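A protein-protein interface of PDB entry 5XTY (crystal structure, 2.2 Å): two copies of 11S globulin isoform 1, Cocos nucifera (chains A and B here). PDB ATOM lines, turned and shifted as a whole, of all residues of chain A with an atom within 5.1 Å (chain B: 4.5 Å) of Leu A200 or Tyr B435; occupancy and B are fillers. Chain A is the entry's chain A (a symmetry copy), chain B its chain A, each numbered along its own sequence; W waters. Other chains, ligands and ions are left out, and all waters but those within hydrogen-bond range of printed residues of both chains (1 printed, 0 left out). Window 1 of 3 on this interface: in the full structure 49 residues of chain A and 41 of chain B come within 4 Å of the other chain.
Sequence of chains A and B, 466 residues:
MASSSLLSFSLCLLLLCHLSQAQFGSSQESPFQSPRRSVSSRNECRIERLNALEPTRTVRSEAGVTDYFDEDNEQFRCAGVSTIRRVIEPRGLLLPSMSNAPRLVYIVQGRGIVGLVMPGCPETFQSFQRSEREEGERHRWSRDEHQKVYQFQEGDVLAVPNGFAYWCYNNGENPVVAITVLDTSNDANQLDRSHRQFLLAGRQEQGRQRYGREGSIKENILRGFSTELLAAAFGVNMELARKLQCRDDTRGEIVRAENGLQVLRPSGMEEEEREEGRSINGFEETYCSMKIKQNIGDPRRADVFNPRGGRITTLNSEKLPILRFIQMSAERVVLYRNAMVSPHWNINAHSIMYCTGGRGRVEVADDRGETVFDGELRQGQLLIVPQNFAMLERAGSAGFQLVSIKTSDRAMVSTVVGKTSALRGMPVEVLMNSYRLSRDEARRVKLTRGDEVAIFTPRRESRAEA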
ATOM      1  N   PRO A  96      -4.572  23.104 -28.793  1.00  0.00           N
ATOM      2  CA  PRO A  96      -4.430  21.742 -28.286  1.00  0.00           C
ATOM      3  C   PRO A  96      -5.552  20.888 -28.827  1.00  0.00           C
ATOM      4  O   PRO A  96      -6.710  21.302 -28.865  1.00  0.00           O
ATOM      5  CB  PRO A  96      -4.536  21.909 -26.768  1.00  0.00           C
ATOM      6  CG  PRO A  96      -4.107  23.284 -26.524  1.00  0.00           C
ATOM      7  CD  PRO A  96      -4.612  24.081 -27.699  1.00  0.00           C
ATOM      8  N   SER A  97      -5.183  19.701 -29.277  1.00  0.00           N
ATOM      9  CA  SER A  97      -6.132  18.718 -29.752  1.00  0.00           C
ATOM     10  C   SER A  97      -5.362  17.443 -29.947  1.00  0.00           C
ATOM     11  O   SER A  97      -4.211  17.478 -30.375  1.00  0.00           O
ATOM     12  CB  SER A  97      -6.789  19.150 -31.060  1.00  0.00           C
ATOM     13  OG  SER A  97      -5.813  19.406 -32.044  1.00  0.00           O
ATOM     14  N   ALA A 165      -1.487  14.678 -27.628  1.00  0.00           N
ATOM     15  CA  ALA A 165      -1.809  16.091 -27.710  1.00  0.00           C
ATOM     16  C   ALA A 165      -0.596  16.895 -28.133  1.00  0.00           C
ATOM     17  O   ALA A 165       0.543  16.582 -27.779  1.00  0.00           O
ATOM     18  CB  ALA A 165      -2.324  16.621 -26.373  1.00  0.00           C
ATOM     19  N   PHE A 198      -9.823  15.578 -31.450  1.00  0.00           N
ATOM     20  CA  PHE A 198     -10.482  15.855 -30.176  1.00  0.00           C
ATOM     21  C   PHE A 198      -9.970  17.195 -29.675  1.00  0.00           C
ATOM     22  O   PHE A 198      -8.872  17.287 -29.125  1.00  0.00           O
ATOM     23  CB  PHE A 198     -10.212  14.736 -29.176  1.00  0.00           C
ATOM     24  CG  PHE A 198     -11.053  13.500 -29.395  1.00  0.00           C
ATOM     25  CD1 PHE A 198     -10.788  12.635 -30.443  1.00  0.00           C
ATOM     26  CD2 PHE A 198     -12.106  13.198 -28.548  1.00  0.00           C
ATOM     27  CE1 PHE A 198     -11.558  11.502 -30.641  1.00  0.00           C
ATOM     28  CE2 PHE A 198     -12.874  12.070 -28.750  1.00  0.00           C
ATOM     29  CZ  PHE A 198     -12.601  11.225 -29.796  1.00  0.00           C
ATOM     30  N   LEU A 199     -10.756  18.248 -29.864  1.00  0.00           N
ATOM     31  CA  LEU A 199     -10.274  19.582 -29.531  1.00  0.00           C
ATOM     32  C   LEU A 199     -10.273  19.774 -28.026  1.00  0.00           C
ATOM     33  O   LEU A 199     -11.325  19.768 -27.391  1.00  0.00           O
ATOM     34  CB  LEU A 199     -11.120  20.647 -30.214  1.00  0.00           C
ATOM     35  CG  LEU A 199     -10.395  21.267 -31.407  1.00  0.00           C
ATOM     36  CD1 LEU A 199      -9.324  22.224 -30.951  1.00  0.00           C
ATOM     37  CD2 LEU A 199      -9.777  20.178 -32.256  1.00  0.00           C
ATOM     38  N   LEU A 200      -9.086  19.927 -27.450  1.00  0.00           N
ATOM     39  CA  LEU A 200      -8.988  20.276 -26.041  1.00  0.00           C
ATOM     40  C   LEU A 200      -9.556  21.657 -25.788  1.00  0.00           C
ATOM     41  O   LEU A 200     -10.285  21.881 -24.816  1.00  0.00           O
ATOM     42  CB  LEU A 200      -7.535  20.238 -25.598  1.00  0.00           C
ATOM     43  CG  LEU A 200      -7.008  18.874 -25.207  1.00  0.00           C
ATOM     44  CD1 LEU A 200      -5.766  19.035 -24.371  1.00  0.00           C
ATOM     45  CD2 LEU A 200      -8.061  18.143 -24.438  1.00  0.00           C
ATOM     46  N   ALA A 201      -9.210  22.601 -26.641  1.00  0.00           N
ATOM     47  CA  ALA A 201      -9.595  23.980 -26.467  1.00  0.00           C
ATOM     48  C   ALA A 201     -10.447  24.419 -27.636  1.00  0.00           C
ATOM     49  O   ALA A 201     -10.486  23.774 -28.679  1.00  0.00           O
ATOM     50  CB  ALA A 201      -8.371  24.879 -26.357  1.00  0.00           C
ATOM     51  N   GLY A 202     -11.163  25.510 -27.422  1.00  0.00           N
ATOM     52  CA  GLY A 202     -11.735  26.282 -28.501  1.00  0.00           C
ATOM     53  C   GLY A 202     -12.543  25.539 -29.534  1.00  0.00           C
ATOM     54  O   GLY A 202     -13.061  24.453 -29.278  1.00  0.00           O
ATOM     55  N   ASN A 220     -14.755  22.194 -28.725  1.00  0.00           N
ATOM     56  CA  ASN A 220     -13.842  21.391 -27.949  1.00  0.00           C
ATOM     57  C   ASN A 220     -14.636  20.422 -27.087  1.00  0.00           C
ATOM     58  O   ASN A 220     -15.864  20.440 -27.052  1.00  0.00           O
ATOM     59  CB  ASN A 220     -12.928  22.272 -27.111  1.00  0.00           C
ATOM     60  CG  ASN A 220     -13.604  22.814 -25.909  1.00  0.00           C
ATOM     61  OD1 ASN A 220     -13.255  22.474 -24.787  1.00  0.00           O
ATOM     62  ND2 ASN A 220     -14.580  23.674 -26.125  1.00  0.00           N
ATOM     63  N   ILE A 221     -13.916  19.556 -26.390  1.00  0.00           N
ATOM     64  CA  ILE A 221     -14.564  18.429 -25.742  1.00  0.00           C
ATOM     65  C   ILE A 221     -15.317  18.860 -24.500  1.00  0.00           C
ATOM     66  O   ILE A 221     -16.422  18.381 -24.234  1.00  0.00           O
ATOM     67  CB  ILE A 221     -13.512  17.381 -25.405  1.00  0.00           C
ATOM     68  CG1 ILE A 221     -12.300  18.100 -24.858  1.00  0.00           C
ATOM     69  CG2 ILE A 221     -13.167  16.609 -26.634  1.00  0.00           C
ATOM     70  CD1 ILE A 221     -11.516  17.279 -23.930  1.00  0.00           C
ATOM     71  N   LEU A 222     -14.731  19.759 -23.714  1.00  0.00           N
ATOM     72  CA  LEU A 222     -15.267  20.066 -22.399  1.00  0.00           C
ATOM     73  C   LEU A 222     -16.645  20.672 -22.454  1.00  0.00           C
ATOM     74  O   LEU A 222     -17.315  20.723 -21.426  1.00  0.00           O
ATOM     75  CB  LEU A 222     -14.322  20.999 -21.675  1.00  0.00           C
ATOM     76  CG  LEU A 222     -12.921  20.415 -21.739  1.00  0.00           C
ATOM     77  CD1 LEU A 222     -11.874  21.500 -21.615  1.00  0.00           C
ATOM     78  CD2 LEU A 222     -12.756  19.381 -20.657  1.00  0.00           C
ATOM     79  N   LYS A 243     -15.979  29.535 -18.946  1.00  0.00           N
ATOM     80  CA  LYS A 243     -14.778  29.943 -19.647  1.00  0.00           C
ATOM     81  C   LYS A 243     -14.214  28.798 -20.443  1.00  0.00           C
ATOM     82  O   LYS A 243     -13.758  28.998 -21.566  1.00  0.00           O
ATOM     83  CB  LYS A 243     -13.725  30.451 -18.663  1.00  0.00           C
ATOM     84  CG  LYS A 243     -13.216  31.850 -18.982  1.00  0.00           C
ATOM     85  CD  LYS A 243     -12.510  32.484 -17.783  1.00  0.00           C
ATOM     86  CE  LYS A 243     -12.032  33.888 -18.090  1.00  0.00           C
ATOM     87  NZ  LYS A 243     -10.797  34.153 -17.344  1.00  0.00           N
ATOM     88  N   LEU A 244     -14.313  27.584 -19.915  1.00  0.00           N
ATOM     89  CA  LEU A 244     -13.591  26.446 -20.464  1.00  0.00           C
ATOM     90  C   LEU A 244     -14.300  25.758 -21.611  1.00  0.00           C
ATOM     91  O   LEU A 244     -13.635  25.206 -22.492  1.00  0.00           O
ATOM     92  CB  LEU A 244     -13.319  25.425 -19.372  1.00  0.00           C
ATOM     93  CG  LEU A 244     -12.379  25.975 -18.306  1.00  0.00           C
ATOM     94  CD1 LEU A 244     -11.516  24.868 -17.753  1.00  0.00           C
ATOM     95  CD2 LEU A 244     -11.505  27.093 -18.842  1.00  0.00           C
ATOM     96  N   CYS A 246     -15.259  27.126 -23.939  1.00  0.00           N
ATOM     97  CA  CYS A 246     -14.910  27.969 -25.073  1.00  0.00           C
ATOM     98  C   CYS A 246     -16.171  28.397 -25.809  1.00  0.00           C
ATOM     99  O   CYS A 246     -16.314  28.187 -27.010  1.00  0.00           O
ATOM    100  CB  CYS A 246     -13.941  27.253 -26.006  1.00  0.00           C
ATOM    101  SG  CYS A 246     -12.542  26.512 -25.155  1.00  0.00           S
ATOM    102  N   ARG A 251     -11.840  32.470 -32.795  1.00  0.00           N
ATOM    103  CA  ARG A 251     -10.532  32.626 -33.406  1.00  0.00           C
ATOM    104  C   ARG A 251     -10.023  31.366 -34.088  1.00  0.00           C
ATOM    105  O   ARG A 251      -8.956  31.406 -34.706  1.00  0.00           O
ATOM    106  CB  ARG A 251      -9.544  33.054 -32.343  1.00  0.00           C
ATOM    107  CG  ARG A 251     -10.143  33.914 -31.273  1.00  0.00           C
ATOM    108  CD  ARG A 251      -9.227  33.939 -30.068  1.00  0.00           C
ATOM    109  NE  ARG A 251      -9.396  32.741 -29.255  1.00  0.00           N
ATOM    110  CZ  ARG A 251      -8.550  32.330 -28.319  1.00  0.00           C
ATOM    111  NH1 ARG A 251      -7.438  32.997 -28.057  1.00  0.00           N
ATOM    112  NH2 ARG A 251      -8.819  31.226 -27.648  1.00  0.00           N
ATOM    113  N   LEU B 431      -1.891  27.734 -21.232  1.00  0.00           N
ATOM    114  CA  LEU B 431      -3.225  27.646 -20.674  1.00  0.00           C
ATOM    115  C   LEU B 431      -3.971  28.968 -20.806  1.00  0.00           C
ATOM    116  O   LEU B 431      -5.189  28.975 -21.000  1.00  0.00           O
ATOM    117  CB  LEU B 431      -3.127  27.183 -19.220  1.00  0.00           C
ATOM    118  CG  LEU B 431      -2.344  25.870 -19.028  1.00  0.00           C
ATOM    119  CD1 LEU B 431      -1.971  25.594 -17.574  1.00  0.00           C
ATOM    120  CD2 LEU B 431      -3.125  24.711 -19.593  1.00  0.00           C
ATOM    121  N   MET B 432      -3.262  30.092 -20.763  1.00  0.00           N
ATOM    122  CA  MET B 432      -3.941  31.382 -20.788  1.00  0.00           C
ATOM    123  C   MET B 432      -4.392  31.793 -22.173  1.00  0.00           C
ATOM    124  O   MET B 432      -5.414  32.466 -22.314  1.00  0.00           O
ATOM    125  CB  MET B 432      -3.029  32.466 -20.252  1.00  0.00           C
ATOM    126  CG  MET B 432      -2.273  32.077 -19.043  1.00  0.00           C
ATOM    127  SD  MET B 432      -1.333  33.496 -18.573  1.00  0.00           S
ATOM    128  CE  MET B 432       0.185  32.737 -18.085  1.00  0.00           C
ATOM    129  N   ASN B 433      -3.634  31.443 -23.195  1.00  0.00           N
ATOM    130  CA  ASN B 433      -3.961  31.912 -24.528  1.00  0.00           C
ATOM    131  C   ASN B 433      -5.079  31.105 -25.159  1.00  0.00           C
ATOM    132  O   ASN B 433      -5.857  31.649 -25.952  1.00  0.00           O
ATOM    133  CB  ASN B 433      -2.704  31.871 -25.375  1.00  0.00           C
ATOM    134  CG  ASN B 433      -1.590  32.710 -24.787  1.00  0.00           C
ATOM    135  OD1 ASN B 433      -1.249  33.763 -25.320  1.00  0.00           O
ATOM    136  ND2 ASN B 433      -1.030  32.262 -23.671  1.00  0.00           N
ATOM    137  N   SER B 434      -5.183  29.824 -24.794  1.00  0.00           N
ATOM    138  CA  SER B 434      -6.136  28.910 -25.419  1.00  0.00           C
ATOM    139  C   SER B 434      -7.559  29.289 -25.071  1.00  0.00           C
ATOM    140  O   SER B 434      -8.446  29.307 -25.931  1.00  0.00           O
ATOM    141  CB  SER B 434      -5.882  27.486 -24.941  1.00  0.00           C
ATOM    142  OG  SER B 434      -4.507  27.259 -24.785  1.00  0.00           O
ATOM    143  N   TYR B 435      -7.801  29.551 -23.798  1.00  0.00           N
ATOM    144  CA  TYR B 435      -9.136  29.824 -23.314  1.00  0.00           C
ATOM    145  C   TYR B 435      -9.327  31.283 -22.920  1.00  0.00           C
ATOM    146  O   TYR B 435     -10.398  31.638 -22.419  1.00  0.00           O
ATOM    147  CB  TYR B 435      -9.444  28.887 -22.138  1.00  0.00           C
ATOM    148  CG  TYR B 435      -9.321  27.398 -22.470  1.00  0.00           C
ATOM    149  CD1 TYR B 435      -8.122  26.718 -22.307  1.00  0.00           C
ATOM    150  CD2 TYR B 435     -10.414  26.678 -22.944  1.00  0.00           C
ATOM    151  CE1 TYR B 435      -8.017  25.371 -22.612  1.00  0.00           C
ATOM    152  CE2 TYR B 435     -10.315  25.333 -23.245  1.00  0.00           C
ATOM    153  CZ  TYR B 435      -9.120  24.687 -23.077  1.00  0.00           C
ATOM    154  OH  TYR B 435      -9.040  23.347 -23.386  1.00  0.00           O
ATOM    155  N   ARG B 436      -8.338  32.145 -23.181  1.00  0.00           N
ATOM    156  CA  ARG B 436      -8.360  33.531 -22.734  1.00  0.00           C
ATOM    157  C   ARG B 436      -8.615  33.596 -21.235  1.00  0.00           C
ATOM    158  O   ARG B 436      -9.722  33.914 -20.796  1.00  0.00           O
ATOM    159  CB  ARG B 436      -9.419  34.344 -23.476  1.00  0.00           C
ATOM    160  CG  ARG B 436      -9.710  33.920 -24.903  1.00  0.00           C
ATOM    161  CD  ARG B 436     -11.198  34.038 -25.190  1.00  0.00           C
ATOM    162  NE  ARG B 436     -11.505  34.172 -26.610  1.00  0.00           N
ATOM    163  CZ  ARG B 436     -12.722  34.398 -27.094  1.00  0.00           C
ATOM    164  NH1 ARG B 436     -13.755  34.515 -26.274  1.00  0.00           N
ATOM    165  NH2 ARG B 436     -12.909  34.515 -28.400  1.00  0.00           N
ATOM    166  N   LEU B 437      -7.614  33.267 -20.438  1.00  0.00           N
ATOM    167  CA  LEU B 437      -7.701  33.464 -19.009  1.00  0.00           C
ATOM    168  C   LEU B 437      -6.432  34.149 -18.555  1.00  0.00           C
ATOM    169  O   LEU B 437      -5.403  34.063 -19.217  1.00  0.00           O
ATOM    170  CB  LEU B 437      -7.825  32.173 -18.244  1.00  0.00           C
ATOM    171  CG  LEU B 437      -8.637  30.994 -18.769  1.00  0.00           C
ATOM    172  CD1 LEU B 437      -8.389  29.753 -17.857  1.00  0.00           C
ATOM    173  CD2 LEU B 437     -10.125  31.305 -18.976  1.00  0.00           C
HETATM  174  O   HOH W   1      -6.536  23.138 -24.516  1.00  0.00           O
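The backbone carbonyl oxygen (O) of Ser B434 sits at hydrogen-bond distance from the guanidinium group (NH2) of Arg A251, at 2.6 Å. The side-chain hydroxyl of Tyr B435 sits close to the backbone NH of Ala A201, at 3.3 Å. The guanidinium group (NH1) of Arg A251 is in hydrogen-bond range of the backbone carbonyl oxygen (O) of Asn B433 (3.0 Å). O of Leu A200 sits close to OH of Tyr B435 (2.4 Å).
The backbone NH (N) of Gly A202 sits at hydrogen-bond distance from the side-chain sulfur (SG) of Cys A246 (2.8 Å). The backbone carbonyl oxygen (O) of Met B432 sits at hydrogen-bond distance from the backbone NH (N) of Leu B437, 3.0 Å away. The side-chain amide oxygen (OD1) of Asn A220 is in hydrogen-bond range of the backbone NH (N) of Leu A222 (3.3 Å). O of Leu A200 sits close to OD1 of Asn A220 (3.0 Å). The backbone NH of Leu A200 is in hydrogen-bond range of the backbone carbonyl oxygen of Pro A96, 3.1 Å away. ND2 of Asn A220 lies within hydrogen-bond range of SG of Cys A246 (3.6 Å).
Among the printed residues, pairs that only touch across the chains: Lys A243 with Leu B437, Cys A246 with Tyr B435, Leu A244 with Tyr B435, Lys A243 with Arg B436, Arg A251 with Arg B436, Leu A222 with Tyr B435 and Ala A201 with Ser B434.
Leu A200 touches just one residue of chain B: Tyr B435 (2.4 Å). Of the printed residues of chain B, Lys A243 touches Arg B436 (3.6 Å) and Leu B437 (2.9 Å). Printed residues of chain A within 4 Å of Asn B433: Arg A251. Of the printed residues of chain B, Ala A201 touches Ser B434 (3.9 Å) and Tyr B435 (3.2 Å). Of the printed residues of chain A, Ser B434 touches Ala A201 and Arg A251. Printed residues of chain B within 4 Å of Leu A222: Tyr B435 (3.8 Å). Pro A96 touches none of the printed residues of chain B. Ala A165 touches none of the printed residues of chain B. The nearest printed residue of chain B that does not touch Leu A200 is Ser B434 (6.9 Å). The nearest residue of chain A that does not touch Tyr B435 is Gly A202 (4.3 Å). The nearest printed residue of chain A that does not touch Leu B437 is Leu A244 (4.2 Å).
Of the 15 printed residues of chain A, 7 touch a printed residue of chain B. Hydrophobic or aromatic side chains of chain A that line the printed part of chain B: Ala A201 and Leu A222. Along chain A the printed residues that touch a printed residue of chain B span positions 200 to 251. Of the 7 printed residues of chain B, 5 touch a printed residue of chain A.
No position is printed for both chains. Of the 11 pairs that touch across the chains among the printed residues, none has its exchanged pair printed and touching as well.
Water W1 lies within hydrogen-bond range of the side-chain hydroxyl (OH) of Tyr B435 and the backbone NH (N) of Ala A201.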
